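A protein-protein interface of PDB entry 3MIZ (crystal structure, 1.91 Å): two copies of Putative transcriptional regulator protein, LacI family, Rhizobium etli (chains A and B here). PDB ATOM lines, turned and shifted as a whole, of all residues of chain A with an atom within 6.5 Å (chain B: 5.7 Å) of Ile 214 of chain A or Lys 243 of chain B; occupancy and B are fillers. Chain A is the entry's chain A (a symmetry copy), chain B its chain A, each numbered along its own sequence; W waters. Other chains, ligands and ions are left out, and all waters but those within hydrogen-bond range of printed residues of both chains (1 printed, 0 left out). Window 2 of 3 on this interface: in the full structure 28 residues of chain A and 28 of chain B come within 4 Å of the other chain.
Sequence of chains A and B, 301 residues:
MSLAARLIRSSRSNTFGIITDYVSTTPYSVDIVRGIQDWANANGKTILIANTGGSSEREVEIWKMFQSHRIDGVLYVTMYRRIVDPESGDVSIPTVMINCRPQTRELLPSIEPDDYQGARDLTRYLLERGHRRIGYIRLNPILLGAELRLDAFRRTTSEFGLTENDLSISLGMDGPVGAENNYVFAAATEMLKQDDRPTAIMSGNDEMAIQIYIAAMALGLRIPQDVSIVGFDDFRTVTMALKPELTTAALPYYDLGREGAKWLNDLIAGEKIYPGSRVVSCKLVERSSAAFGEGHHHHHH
The side-chain amino group (NZ) of Lys 243 of chain B is in salt-bridge range of the side-chain carboxylate (OE1) of Glu 245 of chain B, 3.8 Å away.
OD1 of Asn 182 of chain A lies within hydrogen-bond range of NE2 of Gln 211 of chain A.
The side-chain hydroxyl (OG1) of Thr 189 of chain A is in hydrogen-bond range of the backbone carbonyl oxygen (O) of Phe 185 of chain A, 2.9 Å away.
N of Phe 185 of chain A lies within hydrogen-bond range of OE1 of Gln 211 of chain A.
Met 217 of chain A touches its own counterpart, Met 217 of chain B.
Printed residues of chain B within 4 Å of Ile 210 of chain A: Ala 241 and Leu 242.
Of the printed residues of chain B, Gln 211 of chain A touches Ala 241 (3.1 Å) and Lys 243 (3.6 Å).
Ile 214 of chain A touches three residues of chain B.
Of the printed residues of chain B, Ala 218 of chain A touches Met 217 (3.5 Å).
Of the printed residues of chain A, Met 217 of chain B touches Ile 214, Met 217 and Ala 218.
Of the printed residues of chain A, Ala 241 of chain B touches Ile 210 and Gln 211.
Lys 243 of chain B touches three residues of chain A.
The nearest residue of chain B that does not touch Ile 214 of chain A is Ala 241 of chain B (4.3 Å).
The nearest residue of chain A that does not touch Lys 243 of chain B is Asn 182 of chain A (5.3 Å).
The nearest printed residue of chain B that does not touch Phe 185 of chain A is Ala 241 of chain B (5.7 Å).
Among the printed residues, pairs that only touch across the chains: Phe 185 of chain A with Lys 243 of chain B (3.7 Å), Ile 210 of chain A with Ala 241 of chain B (3.9 Å), Ile 210 of chain A with Leu 242 of chain B (3.8 Å), Gln 211 of chain A with Ala 241 of chain B (3.1 Å), Gln 211 of chain A with Lys 243 of chain B (3.6 Å), Ile 214 of chain A with Met 217 of chain B (3.6 Å), Ile 214 of chain A with Leu 242 of chain B (3.7 Å), Ile 214 of chain A with Lys 243 of chain B (3.4 Å), Met 217 of chain A with Met 217 of chain B (3.9 Å) and Ala 218 of chain A with Met 217 of chain B (3.5 Å).
Water W1 lies within hydrogen-bond range of the side-chain amide oxygen (OE1) of Gln 211 of chain A (2.6 Å), the backbone carbonyl oxygen (O) of Asn 182 of chain A (2.9 Å) and the side-chain amino group (NZ) of Lys 243 of chain B (3.2 Å).
Printed residues of chain B that touch a printed residue of chain A: Met 217, Ala 241, Leu 242 and Lys 243.
Among the printed residues, no Asp or Glu carboxylate lies within 4 Å of a Lys or Arg side-chain nitrogen of the other chain.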
ATOM      1  N   ASN A 182       2.776  21.687 -31.301  1.00  0.00           N
ATOM      2  CA  ASN A 182       2.117  20.819 -30.329  1.00  0.00           C
ATOM      3  C   ASN A 182       0.629  21.106 -30.119  1.00  0.00           C
ATOM      4  O   ASN A 182       0.248  22.203 -29.729  1.00  0.00           O
ATOM      5  CB  ASN A 182       2.886  20.921 -29.008  1.00  0.00           C
ATOM      6  CG  ASN A 182       2.373  19.963 -27.956  1.00  0.00           C
ATOM      7  OD1 ASN A 182       1.193  19.991 -27.603  1.00  0.00           O
ATOM      8  ND2 ASN A 182       3.261  19.109 -27.442  1.00  0.00           N
ATOM      9  N   PHE A 185      -3.506  18.948 -26.337  1.00  0.00           N
ATOM     10  CA  PHE A 185      -4.738  19.353 -25.656  1.00  0.00           C
ATOM     11  C   PHE A 185      -5.929  19.385 -26.617  1.00  0.00           C
ATOM     12  O   PHE A 185      -7.003  18.844 -26.319  1.00  0.00           O
ATOM     13  CB  PHE A 185      -4.570  20.742 -25.031  1.00  0.00           C
ATOM     14  CG  PHE A 185      -5.813  21.257 -24.357  1.00  0.00           C
ATOM     15  CD1 PHE A 185      -6.185  20.793 -23.096  1.00  0.00           C
ATOM     16  CD2 PHE A 185      -6.629  22.188 -24.999  1.00  0.00           C
ATOM     17  CE1 PHE A 185      -7.347  21.243 -22.486  1.00  0.00           C
ATOM     18  CE2 PHE A 185      -7.800  22.648 -24.397  1.00  0.00           C
ATOM     19  CZ  PHE A 185      -8.161  22.173 -23.136  1.00  0.00           C
ATOM     20  N   ALA A 186      -5.735  20.029 -27.765  1.00  0.00           N
ATOM     21  CA  ALA A 186      -6.792  20.152 -28.765  1.00  0.00           C
ATOM     22  C   ALA A 186      -7.205  18.800 -29.328  1.00  0.00           C
ATOM     23  O   ALA A 186      -8.389  18.560 -29.563  1.00  0.00           O
ATOM     24  CB  ALA A 186      -6.346  21.083 -29.898  1.00  0.00           C
ATOM     25  N   THR A 189      -9.121  16.858 -26.641  1.00  0.00           N
ATOM     26  CA  THR A 189     -10.436  17.447 -26.436  1.00  0.00           C
ATOM     27  C   THR A 189     -11.405  16.943 -27.505  1.00  0.00           C
ATOM     28  O   THR A 189     -12.524  16.533 -27.198  1.00  0.00           O
ATOM     29  CB  THR A 189     -10.356  18.980 -26.470  1.00  0.00           C
ATOM     30  OG1 THR A 189      -9.629  19.432 -25.320  1.00  0.00           O
ATOM     31  CG2 THR A 189     -11.757  19.598 -26.447  1.00  0.00           C
ATOM     32  N   ALA A 209       0.666  13.488 -21.316  1.00  0.00           N
ATOM     33  CA  ALA A 209      -0.443  13.189 -20.406  1.00  0.00           C
ATOM     34  C   ALA A 209      -0.906  14.419 -19.647  1.00  0.00           C
ATOM     35  O   ALA A 209      -2.071  14.512 -19.279  1.00  0.00           O
ATOM     36  CB  ALA A 209      -0.052  12.088 -19.419  1.00  0.00           C
ATOM     37  N   ILE A 210       0.003  15.361 -19.400  1.00  0.00           N
ATOM     38  CA  ILE A 210      -0.387  16.570 -18.693  1.00  0.00           C
ATOM     39  C   ILE A 210      -1.546  17.244 -19.432  1.00  0.00           C
ATOM     40  O   ILE A 210      -2.536  17.632 -18.821  1.00  0.00           O
ATOM     41  CB  ILE A 210       0.771  17.587 -18.593  1.00  0.00           C
ATOM     42  CG1 ILE A 210       1.916  17.013 -17.751  1.00  0.00           C
ATOM     43  CG2 ILE A 210       0.263  18.883 -17.939  1.00  0.00           C
ATOM     44  CD1 ILE A 210       3.198  17.849 -17.827  1.00  0.00           C
ATOM     45  N   GLN A 211      -1.414  17.380 -20.749  1.00  0.00           N
ATOM     46  CA  GLN A 211      -2.455  18.024 -21.555  1.00  0.00           C
ATOM     47  C   GLN A 211      -3.744  17.219 -21.644  1.00  0.00           C
ATOM     48  O   GLN A 211      -4.834  17.798 -21.743  1.00  0.00           O
ATOM     49  CB  GLN A 211      -1.929  18.310 -22.964  1.00  0.00           C
ATOM     50  CG  GLN A 211      -0.779  19.307 -22.967  1.00  0.00           C
ATOM     51  CD  GLN A 211      -0.363  19.704 -24.363  1.00  0.00           C
ATOM     52  OE1 GLN A 211      -1.164  20.252 -25.130  1.00  0.00           O
ATOM     53  NE2 GLN A 211       0.892  19.436 -24.704  1.00  0.00           N
ATOM     54  N   ILE A 212      -3.622  15.892 -21.620  1.00  0.00           N
ATOM     55  CA  ILE A 212      -4.786  15.009 -21.686  1.00  0.00           C
ATOM     56  C   ILE A 212      -5.556  15.053 -20.352  1.00  0.00           C
ATOM     57  O   ILE A 212      -6.785  14.968 -20.327  1.00  0.00           O
ATOM     58  CB  ILE A 212      -4.352  13.556 -22.011  1.00  0.00           C
ATOM     59  CG1 ILE A 212      -3.588  13.543 -23.343  1.00  0.00           C
ATOM     60  CG2 ILE A 212      -5.579  12.647 -22.122  1.00  0.00           C
ATOM     61  CD1 ILE A 212      -2.962  12.220 -23.702  1.00  0.00           C
ATOM     62  N   TYR A 213      -4.835  15.169 -19.241  1.00  0.00           N
ATOM     63  CA  TYR A 213      -5.492  15.259 -17.933  1.00  0.00           C
ATOM     64  C   TYR A 213      -6.323  16.533 -17.911  1.00  0.00           C
ATOM     65  O   TYR A 213      -7.483  16.526 -17.500  1.00  0.00           O
ATOM     66  CB  TYR A 213      -4.457  15.341 -16.804  1.00  0.00           C
ATOM     67  CG  TYR A 213      -4.141  14.022 -16.130  1.00  0.00           C
ATOM     68  CD1 TYR A 213      -3.690  12.924 -16.862  1.00  0.00           C
ATOM     69  CD2 TYR A 213      -4.236  13.897 -14.742  1.00  0.00           C
ATOM     70  CE1 TYR A 213      -3.334  11.733 -16.228  1.00  0.00           C
ATOM     71  CE2 TYR A 213      -3.878  12.714 -14.098  1.00  0.00           C
ATOM     72  CZ  TYR A 213      -3.427  11.638 -14.845  1.00  0.00           C
ATOM     73  OH  TYR A 213      -3.053  10.478 -14.207  1.00  0.00           O
ATOM     74  N   ILE A 214      -5.714  17.631 -18.350  1.00  0.00           N
ATOM     75  CA  ILE A 214      -6.390  18.925 -18.360  1.00  0.00           C
ATOM     76  C   ILE A 214      -7.563  18.926 -19.337  1.00  0.00           C
ATOM     77  O   ILE A 214      -8.629  19.469 -19.037  1.00  0.00           O
ATOM     78  CB  ILE A 214      -5.398  20.061 -18.697  1.00  0.00           C
ATOM     79  CG1 ILE A 214      -4.299  20.101 -17.615  1.00  0.00           C
ATOM     80  CG2 ILE A 214      -6.124  21.408 -18.762  1.00  0.00           C
ATOM     81  CD1 ILE A 214      -3.301  21.205 -17.788  1.00  0.00           C
ATOM     82  N   ALA A 215      -7.371  18.303 -20.496  1.00  0.00           N
ATOM     83  CA  ALA A 215      -8.439  18.223 -21.482  1.00  0.00           C
ATOM     84  C   ALA A 215      -9.654  17.502 -20.881  1.00  0.00           C
ATOM     85  O   ALA A 215     -10.786  17.954 -21.014  1.00  0.00           O
ATOM     86  CB  ALA A 215      -7.947  17.480 -22.718  1.00  0.00           C
ATOM     87  N   ALA A 216      -9.412  16.380 -20.216  1.00  0.00           N
ATOM     88  CA  ALA A 216     -10.501  15.609 -19.616  1.00  0.00           C
ATOM     89  C   ALA A 216     -11.207  16.361 -18.484  1.00  0.00           C
ATOM     90  O   ALA A 216     -12.442  16.434 -18.456  1.00  0.00           O
ATOM     91  CB  ALA A 216      -9.973  14.270 -19.110  1.00  0.00           C
ATOM     92  N   MET A 217     -10.433  16.912 -17.553  1.00  0.00           N
ATOM     93  CA  MET A 217     -11.010  17.644 -16.427  1.00  0.00           C
ATOM     94  C   MET A 217     -11.752  18.902 -16.873  1.00  0.00           C
ATOM     95  O   MET A 217     -12.753  19.293 -16.265  1.00  0.00           O
ATOM     96  CB  MET A 217      -9.916  18.013 -15.418  1.00  0.00           C
ATOM     97  CG  MET A 217      -9.256  16.809 -14.790  1.00  0.00           C
ATOM     98  SD  MET A 217      -7.829  17.286 -13.570  1.00  0.00           S
ATOM     99  CE  MET A 217      -8.914  17.590 -11.984  1.00  0.00           C
ATOM    100  N   ALA A 218     -11.270  19.524 -17.943  1.00  0.00           N
ATOM    101  CA  ALA A 218     -11.899  20.728 -18.460  1.00  0.00           C
ATOM    102  C   ALA A 218     -13.287  20.420 -19.020  1.00  0.00           C
ATOM    103  O   ALA A 218     -14.084  21.333 -19.254  1.00  0.00           O
ATOM    104  CB  ALA A 218     -11.022  21.353 -19.542  1.00  0.00           C
ATOM    105  N   LEU A 219     -13.569  19.139 -19.234  1.00  0.00           N
ATOM    106  CA  LEU A 219     -14.867  18.709 -19.760  1.00  0.00           C
ATOM    107  C   LEU A 219     -15.706  18.078 -18.655  1.00  0.00           C
ATOM    108  O   LEU A 219     -16.750  17.482 -18.920  1.00  0.00           O
ATOM    109  CB  LEU A 219     -14.682  17.696 -20.898  1.00  0.00           C
ATOM    110  CG  LEU A 219     -14.048  18.187 -22.203  1.00  0.00           C
ATOM    111  CD1 LEU A 219     -13.773  16.989 -23.107  1.00  0.00           C
ATOM    112  CD2 LEU A 219     -14.974  19.176 -22.894  1.00  0.00           C
ATOM    113  N   ILE A 223     -10.817  11.446 -13.788  1.00  0.00           N
ATOM    114  CA  ILE A 223      -9.868  10.505 -14.360  1.00  0.00           C
ATOM    115  C   ILE A 223     -10.241   9.028 -14.243  1.00  0.00           C
ATOM    116  O   ILE A 223     -11.027   8.534 -15.051  1.00  0.00           O
ATOM    117  CB  ILE A 223      -8.439  10.761 -13.845  1.00  0.00           C
ATOM    118  CG1 ILE A 223      -8.067  12.230 -14.062  1.00  0.00           C
ATOM    119  CG2 ILE A 223      -7.453   9.862 -14.584  1.00  0.00           C
ATOM    120  CD1 ILE A 223      -8.121  12.693 -15.523  1.00  0.00           C
ATOM    121  N   TYR B 213      -2.860  23.273 -10.544  1.00  0.00           N
ATOM    122  CA  TYR B 213      -3.869  23.326 -11.607  1.00  0.00           C
ATOM    123  C   TYR B 213      -4.872  22.209 -11.358  1.00  0.00           C
ATOM    124  O   TYR B 213      -6.082  22.419 -11.421  1.00  0.00           O
ATOM    125  CB  TYR B 213      -3.229  23.101 -12.982  1.00  0.00           C
ATOM    126  CG  TYR B 213      -2.904  24.365 -13.751  1.00  0.00           C
ATOM    127  CD1 TYR B 213      -2.085  25.353 -13.206  1.00  0.00           C
ATOM    128  CD2 TYR B 213      -3.369  24.538 -15.056  1.00  0.00           C
ATOM    129  CE1 TYR B 213      -1.732  26.484 -13.943  1.00  0.00           C
ATOM    130  CE2 TYR B 213      -3.018  25.658 -15.804  1.00  0.00           C
ATOM    131  CZ  TYR B 213      -2.200  26.625 -15.244  1.00  0.00           C
ATOM    132  OH  TYR B 213      -1.835  27.722 -15.991  1.00  0.00           O
ATOM    133  N   MET B 217      -8.915  22.530 -10.517  1.00  0.00           N
ATOM    134  CA  MET B 217      -9.905  21.932 -11.413  1.00  0.00           C
ATOM    135  C   MET B 217     -10.687  20.806 -10.742  1.00  0.00           C
ATOM    136  O   MET B 217     -11.871  20.601 -11.029  1.00  0.00           O
ATOM    137  CB  MET B 217      -9.222  21.411 -12.683  1.00  0.00           C
ATOM    138  CG  MET B 217      -8.578  22.503 -13.503  1.00  0.00           C
ATOM    139  SD  MET B 217      -7.660  21.825 -15.068  1.00  0.00           S
ATOM    140  CE  MET B 217      -9.188  21.745 -16.270  1.00  0.00           C
ATOM    141  N   ILE B 223      -9.443  28.075 -14.148  1.00  0.00           N
ATOM    142  CA  ILE B 223      -8.227  28.829 -13.895  1.00  0.00           C
ATOM    143  C   ILE B 223      -8.366  30.351 -13.936  1.00  0.00           C
ATOM    144  O   ILE B 223      -8.794  30.949 -12.950  1.00  0.00           O
ATOM    145  CB  ILE B 223      -7.068  28.351 -14.791  1.00  0.00           C
ATOM    146  CG1 ILE B 223      -6.900  26.835 -14.654  1.00  0.00           C
ATOM    147  CG2 ILE B 223      -5.777  29.055 -14.387  1.00  0.00           C
ATOM    148  CD1 ILE B 223      -6.611  26.352 -13.226  1.00  0.00           C
ATOM    149  N   MET B 240       4.152  25.254 -21.222  1.00  0.00           N
ATOM    150  CA  MET B 240       3.413  25.100 -22.465  1.00  0.00           C
ATOM    151  C   MET B 240       2.563  23.830 -22.532  1.00  0.00           C
ATOM    152  O   MET B 240       1.931  23.549 -23.556  1.00  0.00           O
ATOM    153  CB  MET B 240       4.378  25.144 -23.643  1.00  0.00           C
ATOM    154  CG  MET B 240       5.042  26.495 -23.812  1.00  0.00           C
ATOM    155  SD  MET B 240       6.195  26.522 -25.337  1.00  0.00           S
ATOM    156  CE  MET B 240       4.897  27.075 -26.670  1.00  0.00           C
ATOM    157  N   ALA B 241       2.555  23.066 -21.444  1.00  0.00           N
ATOM    158  CA  ALA B 241       1.756  21.850 -21.364  1.00  0.00           C
ATOM    159  C   ALA B 241       0.453  22.226 -20.668  1.00  0.00           C
ATOM    160  O   ALA B 241      -0.632  21.815 -21.075  1.00  0.00           O
ATOM    161  CB  ALA B 241       2.491  20.779 -20.557  1.00  0.00           C
ATOM    162  N   LEU B 242       0.569  23.017 -19.610  1.00  0.00           N
ATOM    163  CA  LEU B 242      -0.605  23.447 -18.868  1.00  0.00           C
ATOM    164  C   LEU B 242      -1.457  24.358 -19.743  1.00  0.00           C
ATOM    165  O   LEU B 242      -0.941  25.135 -20.553  1.00  0.00           O
ATOM    166  CB  LEU B 242      -0.197  24.202 -17.598  1.00  0.00           C
ATOM    167  CG  LEU B 242       0.722  23.457 -16.622  1.00  0.00           C
ATOM    168  CD1 LEU B 242       1.135  24.390 -15.493  1.00  0.00           C
ATOM    169  CD2 LEU B 242       0.014  22.220 -16.082  1.00  0.00           C
ATOM    170  N   LYS B 243      -2.767  24.239 -19.582  1.00  0.00           N
ATOM    171  CA  LYS B 243      -3.715  25.064 -20.317  1.00  0.00           C
ATOM    172  C   LYS B 243      -4.687  25.549 -19.252  1.00  0.00           C
ATOM    173  O   LYS B 243      -5.267  24.740 -18.525  1.00  0.00           O
ATOM    174  CB  LYS B 243      -4.469  24.232 -21.364  1.00  0.00           C
ATOM    175  CG  LYS B 243      -3.580  23.480 -22.347  1.00  0.00           C
ATOM    176  CD  LYS B 243      -2.812  24.417 -23.267  1.00  0.00           C
ATOM    177  CE  LYS B 243      -1.948  23.629 -24.245  1.00  0.00           C
ATOM    178  NZ  LYS B 243      -1.209  24.506 -25.194  1.00  0.00           N
ATOM    179  N   PRO B 244      -4.876  26.870 -19.136  1.00  0.00           N
ATOM    180  CA  PRO B 244      -4.244  27.926 -19.938  1.00  0.00           C
ATOM    181  C   PRO B 244      -2.732  28.003 -19.766  1.00  0.00           C
ATOM    182  O   PRO B 244      -2.182  27.561 -18.746  1.00  0.00           O
ATOM    183  CB  PRO B 244      -4.931  29.190 -19.436  1.00  0.00           C
ATOM    184  CG  PRO B 244      -5.139  28.882 -17.985  1.00  0.00           C
ATOM    185  CD  PRO B 244      -5.654  27.454 -18.027  1.00  0.00           C
ATOM    186  N   GLU B 245      -2.063  28.562 -20.775  1.00  0.00           N
ATOM    187  CA  GLU B 245      -0.614  28.726 -20.753  1.00  0.00           C
ATOM    188  C   GLU B 245      -0.238  29.485 -19.478  1.00  0.00           C
ATOM    189  O   GLU B 245      -0.829  30.515 -19.169  1.00  0.00           O
ATOM    190  CB  GLU B 245      -0.158  29.514 -21.985  1.00  0.00           C
ATOM    191  CG  GLU B 245      -0.306  28.767 -23.296  1.00  0.00           C
ATOM    192  CD  GLU B 245       0.658  27.601 -23.413  1.00  0.00           C
ATOM    193  OE1 GLU B 245       0.566  26.666 -22.591  1.00  0.00           O
ATOM    194  OE2 GLU B 245       1.513  27.623 -24.329  1.00  0.00           O
HETATM  195  O   HOH W   1      -1.023  21.993 -27.120  1.00  0.00           O
